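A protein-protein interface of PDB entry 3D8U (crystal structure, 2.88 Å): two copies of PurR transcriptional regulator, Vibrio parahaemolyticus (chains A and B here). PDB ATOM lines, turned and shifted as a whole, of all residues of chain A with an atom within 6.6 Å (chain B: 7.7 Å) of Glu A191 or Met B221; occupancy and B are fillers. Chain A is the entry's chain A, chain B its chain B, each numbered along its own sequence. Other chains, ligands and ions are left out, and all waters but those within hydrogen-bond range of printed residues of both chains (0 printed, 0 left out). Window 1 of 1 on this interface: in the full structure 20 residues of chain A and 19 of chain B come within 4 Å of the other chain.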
ATOM      1  N   PHE A  14     -27.538  -8.896  -3.859  1.00  0.00           N
ATOM      2  CA  PHE A  14     -27.860  -7.556  -4.313  1.00  0.00           C
ATOM      3  C   PHE A  14     -29.317  -7.528  -4.790  1.00  0.00           C
ATOM      4  O   PHE A  14     -30.010  -6.518  -4.646  1.00  0.00           O
ATOM      5  CB  PHE A  14     -26.902  -7.123  -5.426  1.00  0.00           C
ATOM      6  N   LYS A  16     -32.894  -7.400  -5.027  1.00  0.00           N
ATOM      7  CA  LYS A  16     -33.911  -6.938  -4.083  1.00  0.00           C
ATOM      8  C   LYS A  16     -35.035  -7.962  -3.945  1.00  0.00           C
ATOM      9  O   LYS A  16     -35.669  -8.052  -2.901  1.00  0.00           O
ATOM     10  CB  LYS A  16     -34.448  -5.564  -4.501  1.00  0.00           C
ATOM     11  CG  LYS A  16     -33.332  -4.563  -4.833  1.00  0.00           C
ATOM     12  CD  LYS A  16     -33.745  -3.101  -4.773  1.00  0.00           C
ATOM     13  CE  LYS A  16     -32.579  -2.229  -5.270  1.00  0.00           C
ATOM     14  NZ  LYS A  16     -32.565  -0.786  -4.812  1.00  0.00           N
ATOM     15  N   PRO A 163     -26.451  -3.093 -11.591  1.00  0.00           N
ATOM     16  CA  PRO A 163     -27.028  -1.754 -11.570  1.00  0.00           C
ATOM     17  C   PRO A 163     -26.225  -0.828 -10.691  1.00  0.00           C
ATOM     18  O   PRO A 163     -25.991  -1.165  -9.556  1.00  0.00           O
ATOM     19  CB  PRO A 163     -28.371  -1.991 -10.895  1.00  0.00           C
ATOM     20  CG  PRO A 163     -28.199  -3.296 -10.170  1.00  0.00           C
ATOM     21  CD  PRO A 163     -27.421  -4.086 -11.112  1.00  0.00           C
ATOM     22  N   SER A 164     -25.789   0.317 -11.205  1.00  0.00           N
ATOM     23  CA  SER A 164     -25.068   1.306 -10.387  1.00  0.00           C
ATOM     24  C   SER A 164     -25.521   2.727 -10.736  1.00  0.00           C
ATOM     25  O   SER A 164     -25.877   3.022 -11.888  1.00  0.00           O
ATOM     26  CB  SER A 164     -23.578   1.191 -10.644  1.00  0.00           C
ATOM     27  OG  SER A 164     -23.255   1.770 -11.901  1.00  0.00           O
ATOM     28  N   SER A 165     -25.480   3.622  -9.760  1.00  0.00           N
ATOM     29  CA  SER A 165     -25.833   5.022 -10.013  1.00  0.00           C
ATOM     30  C   SER A 165     -24.928   5.659 -11.079  1.00  0.00           C
ATOM     31  O   SER A 165     -25.429   6.368 -11.971  1.00  0.00           O
ATOM     32  CB  SER A 165     -25.818   5.835  -8.723  1.00  0.00           C
ATOM     33  OG  SER A 165     -24.555   5.732  -8.146  1.00  0.00           O
ATOM     34  N   GLN A 166     -23.620   5.379 -11.009  1.00  0.00           N
ATOM     35  CA  GLN A 166     -22.695   5.807 -12.065  1.00  0.00           C
ATOM     36  C   GLN A 166     -23.301   5.519 -13.428  1.00  0.00           C
ATOM     37  O   GLN A 166     -23.426   6.430 -14.259  1.00  0.00           O
ATOM     38  CB  GLN A 166     -21.343   5.127 -11.936  1.00  0.00           C
ATOM     39  CG  GLN A 166     -20.456   5.286 -13.177  1.00  0.00           C
ATOM     40  CD  GLN A 166     -18.990   4.930 -12.911  1.00  0.00           C
ATOM     41  OE1 GLN A 166     -18.677   3.983 -12.162  1.00  0.00           O
ATOM     42  NE2 GLN A 166     -18.079   5.697 -13.515  1.00  0.00           N
ATOM     43  N   GLY A 168     -26.374   5.050 -14.204  1.00  0.00           N
ATOM     44  CA  GLY A 168     -27.586   5.840 -14.389  1.00  0.00           C
ATOM     45  C   GLY A 168     -27.154   7.199 -14.857  1.00  0.00           C
ATOM     46  O   GLY A 168     -27.677   7.711 -15.840  1.00  0.00           O
ATOM     47  N   ALA A 169     -26.158   7.769 -14.182  1.00  0.00           N
ATOM     48  CA  ALA A 169     -25.704   9.130 -14.505  1.00  0.00           C
ATOM     49  C   ALA A 169     -25.009   9.170 -15.867  1.00  0.00           C
ATOM     50  O   ALA A 169     -25.366   9.967 -16.716  1.00  0.00           O
ATOM     51  CB  ALA A 169     -24.823   9.708 -13.405  1.00  0.00           C
ATOM     52  N   SER A 188     -34.032   0.141 -15.373  1.00  0.00           N
ATOM     53  CA  SER A 188     -34.260  -1.250 -15.003  1.00  0.00           C
ATOM     54  C   SER A 188     -34.201  -1.484 -13.501  1.00  0.00           C
ATOM     55  O   SER A 188     -34.940  -2.331 -12.976  1.00  0.00           O
ATOM     56  CB  SER A 188     -33.227  -2.138 -15.679  1.00  0.00           C
ATOM     57  OG  SER A 188     -31.954  -1.970 -15.079  1.00  0.00           O
ATOM     58  N   HIS A 189     -33.307  -0.762 -12.821  1.00  0.00           N
ATOM     59  CA  HIS A 189     -33.076  -0.930 -11.389  1.00  0.00           C
ATOM     60  C   HIS A 189     -32.976   0.427 -10.727  1.00  0.00           C
ATOM     61  O   HIS A 189     -32.459   1.371 -11.325  1.00  0.00           O
ATOM     62  CB  HIS A 189     -31.747  -1.620 -11.098  1.00  0.00           C
ATOM     63  CG  HIS A 189     -31.622  -3.011 -11.626  1.00  0.00           C
ATOM     64  ND1 HIS A 189     -31.671  -3.312 -12.970  1.00  0.00           N
ATOM     65  CD2 HIS A 189     -31.359  -4.175 -10.990  1.00  0.00           C
ATOM     66  CE1 HIS A 189     -31.492  -4.608 -13.131  1.00  0.00           C
ATOM     67  NE2 HIS A 189     -31.287  -5.153 -11.946  1.00  0.00           N
ATOM     68  N   GLU A 190     -33.398   0.474  -9.463  1.00  0.00           N
ATOM     69  CA  GLU A 190     -33.419   1.658  -8.621  1.00  0.00           C
ATOM     70  C   GLU A 190     -32.106   2.454  -8.439  1.00  0.00           C
ATOM     71  O   GLU A 190     -32.127   3.690  -8.353  1.00  0.00           O
ATOM     72  CB  GLU A 190     -33.934   1.204  -7.263  1.00  0.00           C
ATOM     73  CG  GLU A 190     -34.200   2.316  -6.279  1.00  0.00           C
ATOM     74  CD  GLU A 190     -34.832   1.805  -5.019  1.00  0.00           C
ATOM     75  OE1 GLU A 190     -34.135   1.103  -4.230  1.00  0.00           O
ATOM     76  OE2 GLU A 190     -36.033   2.127  -4.829  1.00  0.00           O
ATOM     77  N   GLU A 191     -30.983   1.750  -8.332  1.00  0.00           N
ATOM     78  CA  GLU A 191     -29.667   2.394  -8.327  1.00  0.00           C
ATOM     79  C   GLU A 191     -29.462   3.277  -9.597  1.00  0.00           C
ATOM     80  O   GLU A 191     -28.978   4.404  -9.515  1.00  0.00           O
ATOM     81  CB  GLU A 191     -28.521   1.355  -8.202  1.00  0.00           C
ATOM     82  CG  GLU A 191     -28.618   0.257  -7.084  1.00  0.00           C
ATOM     83  CD  GLU A 191     -29.481  -0.974  -7.479  1.00  0.00           C
ATOM     84  OE1 GLU A 191     -30.319  -0.907  -8.416  1.00  0.00           O
ATOM     85  OE2 GLU A 191     -29.331  -2.028  -6.831  1.00  0.00           O
ATOM     86  N   ILE A 192     -29.837   2.773 -10.767  1.00  0.00           N
ATOM     87  CA  ILE A 192     -29.717   3.535 -12.012  1.00  0.00           C
ATOM     88  C   ILE A 192     -30.563   4.831 -11.973  1.00  0.00           C
ATOM     89  O   ILE A 192     -30.132   5.916 -12.420  1.00  0.00           O
ATOM     90  CB  ILE A 192     -30.134   2.653 -13.213  1.00  0.00           C
ATOM     91  CG1 ILE A 192     -29.149   1.514 -13.390  1.00  0.00           C
ATOM     92  CG2 ILE A 192     -30.133   3.410 -14.491  1.00  0.00           C
ATOM     93  CD1 ILE A 192     -29.778   0.281 -13.937  1.00  0.00           C
ATOM     94  N   ALA A 193     -31.778   4.713 -11.448  1.00  0.00           N
ATOM     95  CA  ALA A 193     -32.674   5.849 -11.386  1.00  0.00           C
ATOM     96  C   ALA A 193     -32.097   6.940 -10.486  1.00  0.00           C
ATOM     97  O   ALA A 193     -32.238   8.133 -10.776  1.00  0.00           O
ATOM     98  CB  ALA A 193     -34.023   5.413 -10.891  1.00  0.00           C
ATOM     99  N   ILE A 194     -31.442   6.544  -9.400  1.00  0.00           N
ATOM    100  CA  ILE A 194     -30.965   7.540  -8.466  1.00  0.00           C
ATOM    101  C   ILE A 194     -29.799   8.312  -9.071  1.00  0.00           C
ATOM    102  O   ILE A 194     -29.730   9.530  -8.876  1.00  0.00           O
ATOM    103  CB  ILE A 194     -30.602   6.920  -7.105  1.00  0.00           C
ATOM    104  CG1 ILE A 194     -31.872   6.346  -6.455  1.00  0.00           C
ATOM    105  CG2 ILE A 194     -29.865   7.912  -6.218  1.00  0.00           C
ATOM    106  CD1 ILE A 194     -32.834   7.362  -5.807  1.00  0.00           C
ATOM    107  N   GLY A 195     -28.902   7.608  -9.795  1.00  0.00           N
ATOM    108  CA  GLY A 195     -27.797   8.227 -10.504  1.00  0.00           C
ATOM    109  C   GLY A 195     -28.382   9.237 -11.465  1.00  0.00           C
ATOM    110  O   GLY A 195     -28.153  10.444 -11.364  1.00  0.00           O
ATOM    111  N   ALA A 196     -29.184   8.741 -12.387  1.00  0.00           N
ATOM    112  CA  ALA A 196     -29.938   9.584 -13.291  1.00  0.00           C
ATOM    113  C   ALA A 196     -30.577  10.826 -12.595  1.00  0.00           C
ATOM    114  O   ALA A 196     -30.608  11.946 -13.143  1.00  0.00           O
ATOM    115  CB  ALA A 196     -31.000   8.738 -13.976  1.00  0.00           C
ATOM    116  N   PHE A 198     -29.723  12.406  -9.612  1.00  0.00           N
ATOM    117  CA  PHE A 198     -28.563  13.233  -9.384  1.00  0.00           C
ATOM    118  C   PHE A 198     -27.943  13.857 -10.635  1.00  0.00           C
ATOM    119  O   PHE A 198     -27.557  15.026 -10.601  1.00  0.00           O
ATOM    120  CB  PHE A 198     -27.523  12.414  -8.639  1.00  0.00           C
ATOM    121  CG  PHE A 198     -27.819  12.245  -7.189  1.00  0.00           C
ATOM    122  CD1 PHE A 198     -28.192  13.335  -6.410  1.00  0.00           C
ATOM    123  CD2 PHE A 198     -27.704  11.007  -6.587  1.00  0.00           C
ATOM    124  CE1 PHE A 198     -28.463  13.187  -5.061  1.00  0.00           C
ATOM    125  CE2 PHE A 198     -27.953  10.847  -5.205  1.00  0.00           C
ATOM    126  CZ  PHE A 198     -28.337  11.938  -4.450  1.00  0.00           C
ATOM    127  N   CYS A 215     -38.848   3.875 -12.548  1.00  0.00           N
ATOM    128  CA  CYS A 215     -38.116   2.674 -12.181  1.00  0.00           C
ATOM    129  C   CYS A 215     -38.933   1.383 -12.341  1.00  0.00           C
ATOM    130  O   CYS A 215     -40.117   1.339 -11.982  1.00  0.00           O
ATOM    131  CB  CYS A 215     -37.665   2.811 -10.726  1.00  0.00           C
ATOM    132  SG  CYS A 215     -36.479   1.589 -10.148  1.00  0.00           S
ATOM    133  N   GLU A 217     -38.163  -1.681 -10.769  1.00  0.00           N
ATOM    134  CA  GLU A 217     -38.158  -2.559  -9.620  1.00  0.00           C
ATOM    135  C   GLU A 217     -37.765  -1.705  -8.447  1.00  0.00           C
ATOM    136  O   GLU A 217     -36.584  -1.668  -8.061  1.00  0.00           O
ATOM    137  CB  GLU A 217     -37.163  -3.706  -9.824  1.00  0.00           C
ATOM    138  CG  GLU A 217     -37.076  -4.719  -8.673  1.00  0.00           C
ATOM    139  CD  GLU A 217     -35.647  -5.193  -8.380  1.00  0.00           C
ATOM    140  OE1 GLU A 217     -34.678  -4.368  -8.442  1.00  0.00           O
ATOM    141  OE2 GLU A 217     -35.496  -6.402  -8.061  1.00  0.00           O
ATOM    142  N   MET A 221     -36.356   3.471  -1.320  1.00  0.00           N
ATOM    143  CA  MET A 221     -35.313   4.421  -1.631  1.00  0.00           C
ATOM    144  C   MET A 221     -35.737   5.498  -2.606  1.00  0.00           C
ATOM    145  O   MET A 221     -35.551   6.691  -2.347  1.00  0.00           O
ATOM    146  CB  MET A 221     -34.085   3.717  -2.116  1.00  0.00           C
ATOM    147  CG  MET A 221     -33.000   3.769  -1.082  1.00  0.00           C
ATOM    148  SD  MET A 221     -31.437   4.544  -1.939  1.00  0.00           S
ATOM    149  CE  MET A 221     -31.767   3.998  -3.798  1.00  0.00           C
ATOM    150  N   LYS B  16     -24.250  -4.239   3.786  1.00  0.00           N
ATOM    151  CA  LYS B  16     -22.978  -4.177   3.051  1.00  0.00           C
ATOM    152  C   LYS B  16     -21.957  -5.193   3.563  1.00  0.00           C
ATOM    153  O   LYS B  16     -21.422  -5.992   2.793  1.00  0.00           O
ATOM    154  CB  LYS B  16     -22.378  -2.762   3.150  1.00  0.00           C
ATOM    155  CG  LYS B  16     -22.852  -1.739   2.108  1.00  0.00           C
ATOM    156  CD  LYS B  16     -24.311  -1.297   2.287  1.00  0.00           C
ATOM    157  CE  LYS B  16     -24.536   0.091   1.692  1.00  0.00           C
ATOM    158  NZ  LYS B  16     -25.980   0.487   1.705  1.00  0.00           N
ATOM    159  N   GLU B 190     -25.352   4.667   4.274  1.00  0.00           N
ATOM    160  CA  GLU B 190     -25.386   5.343   2.994  1.00  0.00           C
ATOM    161  C   GLU B 190     -26.785   5.707   2.533  1.00  0.00           C
ATOM    162  O   GLU B 190     -26.970   6.771   1.945  1.00  0.00           O
ATOM    163  CB  GLU B 190     -24.669   4.503   1.956  1.00  0.00           C
ATOM    164  CG  GLU B 190     -24.171   5.261   0.765  1.00  0.00           C
ATOM    165  CD  GLU B 190     -23.804   4.322  -0.325  1.00  0.00           C
ATOM    166  OE1 GLU B 190     -24.542   3.316  -0.509  1.00  0.00           O
ATOM    167  OE2 GLU B 190     -22.769   4.567  -0.985  1.00  0.00           O
ATOM    168  N   GLU B 191     -27.763   4.838   2.797  1.00  0.00           N
ATOM    169  CA  GLU B 191     -29.201   5.185   2.540  1.00  0.00           C
ATOM    170  C   GLU B 191     -29.602   6.474   3.256  1.00  0.00           C
ATOM    171  O   GLU B 191     -30.235   7.347   2.684  1.00  0.00           O
ATOM    172  CB  GLU B 191     -30.139   4.075   2.975  1.00  0.00           C
ATOM    173  CG  GLU B 191     -29.884   2.795   2.263  1.00  0.00           C
ATOM    174  CD  GLU B 191     -29.360   1.682   3.164  1.00  0.00           C
ATOM    175  OE1 GLU B 191     -28.343   1.850   3.905  1.00  0.00           O
ATOM    176  OE2 GLU B 191     -29.996   0.601   3.089  1.00  0.00           O
ATOM    177  N   ILE B 194     -28.174   9.572   1.760  1.00  0.00           N
ATOM    178  CA  ILE B 194     -28.789   9.871   0.484  1.00  0.00           C
ATOM    179  C   ILE B 194     -30.107  10.602   0.729  1.00  0.00           C
ATOM    180  O   ILE B 194     -30.406  11.630   0.081  1.00  0.00           O
ATOM    181  CB  ILE B 194     -29.020   8.599  -0.306  1.00  0.00           C
ATOM    182  CG1 ILE B 194     -27.679   8.105  -0.833  1.00  0.00           C
ATOM    183  CG2 ILE B 194     -29.967   8.839  -1.434  1.00  0.00           C
ATOM    184  CD1 ILE B 194     -27.187   8.808  -2.102  1.00  0.00           C
ATOM    185  N   PHE B 198     -30.642  14.432  -0.870  1.00  0.00           N
ATOM    186  CA  PHE B 198     -31.842  14.717  -1.590  1.00  0.00           C
ATOM    187  C   PHE B 198     -32.716  15.730  -0.859  1.00  0.00           C
ATOM    188  O   PHE B 198     -33.318  16.581  -1.506  1.00  0.00           O
ATOM    189  CB  PHE B 198     -32.604  13.428  -1.792  1.00  0.00           C
ATOM    190  CG  PHE B 198     -32.212  12.677  -3.022  1.00  0.00           C
ATOM    191  CD1 PHE B 198     -31.899  13.353  -4.208  1.00  0.00           C
ATOM    192  CD2 PHE B 198     -32.218  11.283  -3.033  1.00  0.00           C
ATOM    193  CE1 PHE B 198     -31.562  12.647  -5.373  1.00  0.00           C
ATOM    194  CE2 PHE B 198     -31.887  10.559  -4.211  1.00  0.00           C
ATOM    195  CZ  PHE B 198     -31.558  11.242  -5.368  1.00  0.00           C
ATOM    196  N   GLY B 218     -19.875   4.315   3.095  1.00  0.00           N
ATOM    197  CA  GLY B 218     -20.200   4.558   1.684  1.00  0.00           C
ATOM    198  C   GLY B 218     -19.843   3.424   0.739  1.00  0.00           C
ATOM    199  O   GLY B 218     -19.059   2.536   1.049  1.00  0.00           O
ATOM    200  N   SER B 219     -20.455   3.456  -0.422  1.00  0.00           N
ATOM    201  CA  SER B 219     -20.164   2.539  -1.486  1.00  0.00           C
ATOM    202  C   SER B 219     -20.107   3.415  -2.729  1.00  0.00           C
ATOM    203  O   SER B 219     -20.280   4.636  -2.647  1.00  0.00           O
ATOM    204  CB  SER B 219     -21.323   1.555  -1.621  1.00  0.00           C
ATOM    205  OG  SER B 219     -22.331   2.036  -2.520  1.00  0.00           O
ATOM    206  N   SER B 220     -19.935   2.801  -3.888  1.00  0.00           N
ATOM    207  CA  SER B 220     -19.977   3.551  -5.135  1.00  0.00           C
ATOM    208  C   SER B 220     -21.291   4.295  -5.280  1.00  0.00           C
ATOM    209  O   SER B 220     -21.388   5.256  -6.044  1.00  0.00           O
ATOM    210  CB  SER B 220     -19.801   2.603  -6.308  1.00  0.00           C
ATOM    211  OG  SER B 220     -20.896   1.719  -6.317  1.00  0.00           O
ATOM    212  N   MET B 221     -22.297   3.854  -4.533  1.00  0.00           N
ATOM    213  CA  MET B 221     -23.637   4.458  -4.608  1.00  0.00           C
ATOM    214  C   MET B 221     -23.558   5.919  -4.299  1.00  0.00           C
ATOM    215  O   MET B 221     -23.987   6.742  -5.081  1.00  0.00           O
ATOM    216  CB  MET B 221     -24.605   3.752  -3.665  1.00  0.00           C
ATOM    217  CG  MET B 221     -25.692   4.611  -3.102  1.00  0.00           C
ATOM    218  SD  MET B 221     -27.267   4.877  -4.211  1.00  0.00           S
ATOM    219  CE  MET B 221     -27.792   3.006  -4.554  1.00  0.00           C
ATOM    220  N   GLY B 222     -22.946   6.213  -3.156  1.00  0.00           N
ATOM    221  CA  GLY B 222     -22.809   7.545  -2.645  1.00  0.00           C
ATOM    222  C   GLY B 222     -21.727   8.254  -3.390  1.00  0.00           C
ATOM    223  O   GLY B 222     -21.819   9.441  -3.582  1.00  0.00           O
ATOM    224  N   GLU B 223     -20.696   7.532  -3.814  1.00  0.00           N
ATOM    225  CA  GLU B 223     -19.603   8.117  -4.610  1.00  0.00           C
ATOM    226  C   GLU B 223     -20.103   8.869  -5.833  1.00  0.00           C
ATOM    227  O   GLU B 223     -19.454   9.809  -6.291  1.00  0.00           O
ATOM    228  CB  GLU B 223     -18.647   7.033  -5.099  1.00  0.00           C
ATOM    229  CG  GLU B 223     -17.505   7.594  -5.911  1.00  0.00           C
ATOM    230  CD  GLU B 223     -16.724   6.525  -6.620  1.00  0.00           C
ATOM    231  OE1 GLU B 223     -17.165   5.360  -6.518  1.00  0.00           O
ATOM    232  OE2 GLU B 223     -15.686   6.834  -7.276  1.00  0.00           O
ATOM    233  N   HIS B 224     -21.238   8.435  -6.375  1.00  0.00           N
ATOM    234  CA  HIS B 224     -21.706   8.995  -7.606  1.00  0.00           C
ATOM    235  C   HIS B 224     -23.032   9.696  -7.440  1.00  0.00           C
ATOM    236  O   HIS B 224     -23.818   9.768  -8.390  1.00  0.00           O
ATOM    237  CB  HIS B 224     -21.804   7.917  -8.672  1.00  0.00           C
ATOM    238  CG  HIS B 224     -20.520   7.657  -9.388  1.00  0.00           C
ATOM    239  ND1 HIS B 224     -19.581   6.756  -8.931  1.00  0.00           N
ATOM    240  CD2 HIS B 224     -20.017   8.180 -10.529  1.00  0.00           C
ATOM    241  CE1 HIS B 224     -18.558   6.728  -9.762  1.00  0.00           C
ATOM    242  NE2 HIS B 224     -18.795   7.589 -10.737  1.00  0.00           N
ATOM    243  N   ALA B 225     -23.292  10.196  -6.235  1.00  0.00           N
ATOM    244  CA  ALA B 225     -24.394  11.122  -6.001  1.00  0.00           C
ATOM    245  C   ALA B 225     -23.945  12.545  -6.396  1.00  0.00           C
ATOM    246  O   ALA B 225     -22.843  12.717  -6.884  1.00  0.00           O
ATOM    247  CB  ALA B 225     -24.763  11.072  -4.580  1.00  0.00           C
ATOM    248  N   TYR B 226     -24.786  13.555  -6.221  1.00  0.00           N
ATOM    249  CA  TYR B 226     -24.396  14.935  -6.506  1.00  0.00           C
ATOM    250  C   TYR B 226     -24.926  15.920  -5.469  1.00  0.00           C
ATOM    251  O   TYR B 226     -26.128  15.960  -5.238  1.00  0.00           O
ATOM    252  CB  TYR B 226     -24.944  15.386  -7.838  1.00  0.00           C
ATOM    253  CG  TYR B 226     -24.695  16.860  -8.076  1.00  0.00           C
ATOM    254  CD1 TYR B 226     -25.686  17.809  -7.806  1.00  0.00           C
ATOM    255  CD2 TYR B 226     -23.455  17.309  -8.556  1.00  0.00           C
ATOM    256  CE1 TYR B 226     -25.457  19.163  -8.017  1.00  0.00           C
ATOM    257  CE2 TYR B 226     -23.215  18.660  -8.778  1.00  0.00           C
ATOM    258  CZ  TYR B 226     -24.222  19.575  -8.503  1.00  0.00           C
ATOM    259  OH  TYR B 226     -23.987  20.907  -8.704  1.00  0.00           O
ATOM    260  N   SER B 228     -21.140  14.654  -4.859  1.00  0.00           N
ATOM    261  CA  SER B 228     -20.727  13.328  -4.421  1.00  0.00           C
ATOM    262  C   SER B 228     -20.372  13.433  -2.972  1.00  0.00           C
ATOM    263  O   SER B 228     -19.954  14.502  -2.521  1.00  0.00           O
ATOM    264  CB  SER B 228     -19.466  12.944  -5.146  1.00  0.00           C
ATOM    265  OG  SER B 228     -18.515  13.974  -4.984  1.00  0.00           O
ATOM    266  N   LEU B 229     -20.477  12.351  -2.214  1.00  0.00           N
ATOM    267  CA  LEU B 229     -20.252  12.565  -0.796  1.00  0.00           C
ATOM    268  C   LEU B 229     -19.099  11.879  -0.109  1.00  0.00           C
ATOM    269  O   LEU B 229     -18.868  10.684  -0.259  1.00  0.00           O
ATOM    270  CB  LEU B 229     -21.554  12.431   0.021  1.00  0.00           C
ATOM    271  CG  LEU B 229     -22.672  11.493  -0.407  1.00  0.00           C
ATOM    272  CD1 LEU B 229     -22.116  10.079  -0.437  1.00  0.00           C
ATOM    273  CD2 LEU B 229     -23.838  11.667   0.566  1.00  0.00           C
ATOM    274  N   GLU B 233     -14.947   4.147   3.690  1.00  0.00           N
ATOM    275  CA  GLU B 233     -15.152   2.914   2.960  1.00  0.00           C
ATOM    276  C   GLU B 233     -14.410   1.786   3.606  1.00  0.00           C
ATOM    277  O   GLU B 233     -13.467   2.029   4.332  1.00  0.00           O
ATOM    278  CB  GLU B 233     -14.734   3.087   1.514  1.00  0.00           C
ATOM    279  CG  GLU B 233     -15.711   3.958   0.740  1.00  0.00           C
ATOM    280  CD  GLU B 233     -15.339   4.063  -0.695  1.00  0.00           C
ATOM    281  OE1 GLU B 233     -14.466   3.299  -1.133  1.00  0.00           O
ATOM    282  OE2 GLU B 233     -15.911   4.907  -1.395  1.00  0.00           O
ATOM    283  N   ARG B 269     -14.737  13.825  -0.613  1.00  0.00           N
ATOM    284  CA  ARG B 269     -15.381  14.291  -1.858  1.00  0.00           C
ATOM    285  C   ARG B 269     -16.100  15.617  -1.654  1.00  0.00           C
ATOM    286  O   ARG B 269     -15.780  16.344  -0.719  1.00  0.00           O
ATOM    287  CB  ARG B 269     -16.371  13.273  -2.403  1.00  0.00           C
ATOM    288  CG  ARG B 269     -16.033  11.872  -2.085  1.00  0.00           C
ATOM    289  CD  ARG B 269     -17.035  11.057  -2.784  1.00  0.00           C
ATOM    290  NE  ARG B 269     -17.159   9.705  -2.254  1.00  0.00           N
ATOM    291  CZ  ARG B 269     -16.396   8.685  -2.627  1.00  0.00           C
ATOM    292  NH1 ARG B 269     -15.425   8.863  -3.524  1.00  0.00           N
ATOM    293  NH2 ARG B 269     -16.621   7.493  -2.097  1.00  0.00           N
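Glu A191 touches Met B221, but with the chains exchanged Met A221 does not touch Glu B191 (4.7 Å). Ile A194 touches Phe B198, and with the chains exchanged Phe A198 touches Ile B194. Phe B198 touches its own counterpart, Phe A198. 6 positions are printed for both chains. Of the 10 pairs that touch across the chains among the printed residues, 3 have their exchanged pair printed and touching as well.
OG of Ser A165 is in hydrogen-bond range of O of Met B221 (3.3 Å). NE2 of His B224 lies within hydrogen-bond range of NE2 of Gln A166 (3.4 Å).
Of the printed residues of chain B, Glu A191 touches Met B221. Of the printed residues of chain B, Ile A194 touches Phe B198 (3.7 Å). Printed residues of chain B within 4 Å of Phe A198: Ile B194 (3.8 Å), Phe B198 (3.2 Å), Ala B225 (3.3 Å) and Tyr B226 (3.4 Å). Printed residues of chain A within 4 Å of Met B221: Ser A165 and Glu A191. Of the printed residues of chain A, Ala B225 touches Phe A198. The nearest residue of chain B that does not touch Glu A191 is His B224 (7.5 Å).
Among the printed residues, merely in contact across the chains: Phe A198 with Phe B198, Phe A198 with Ala B225, Phe A198 with Tyr B226, Ser A165 with His B224, Ile A194 with Phe B198, Phe A198 with Ile B194, Glu A191 with Met B221 and Ser A165 with Ser B220.
Of the 18 printed residues of chain B, 7 touch a printed residue of chain A. Hydrophobic or aromatic side chains of chain B within 4 Å of the printed part of chain A: Ile B194, Phe B198, Met B221, His B224, Ala B225 and Tyr B226. Among the printed residues, 10 pairs touch across the chains.
The side-chain hydroxyl (OG) of Ser B219 sits at hydrogen-bond distance from the backbone NH (N) of Met B221, 2.7 Å away.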
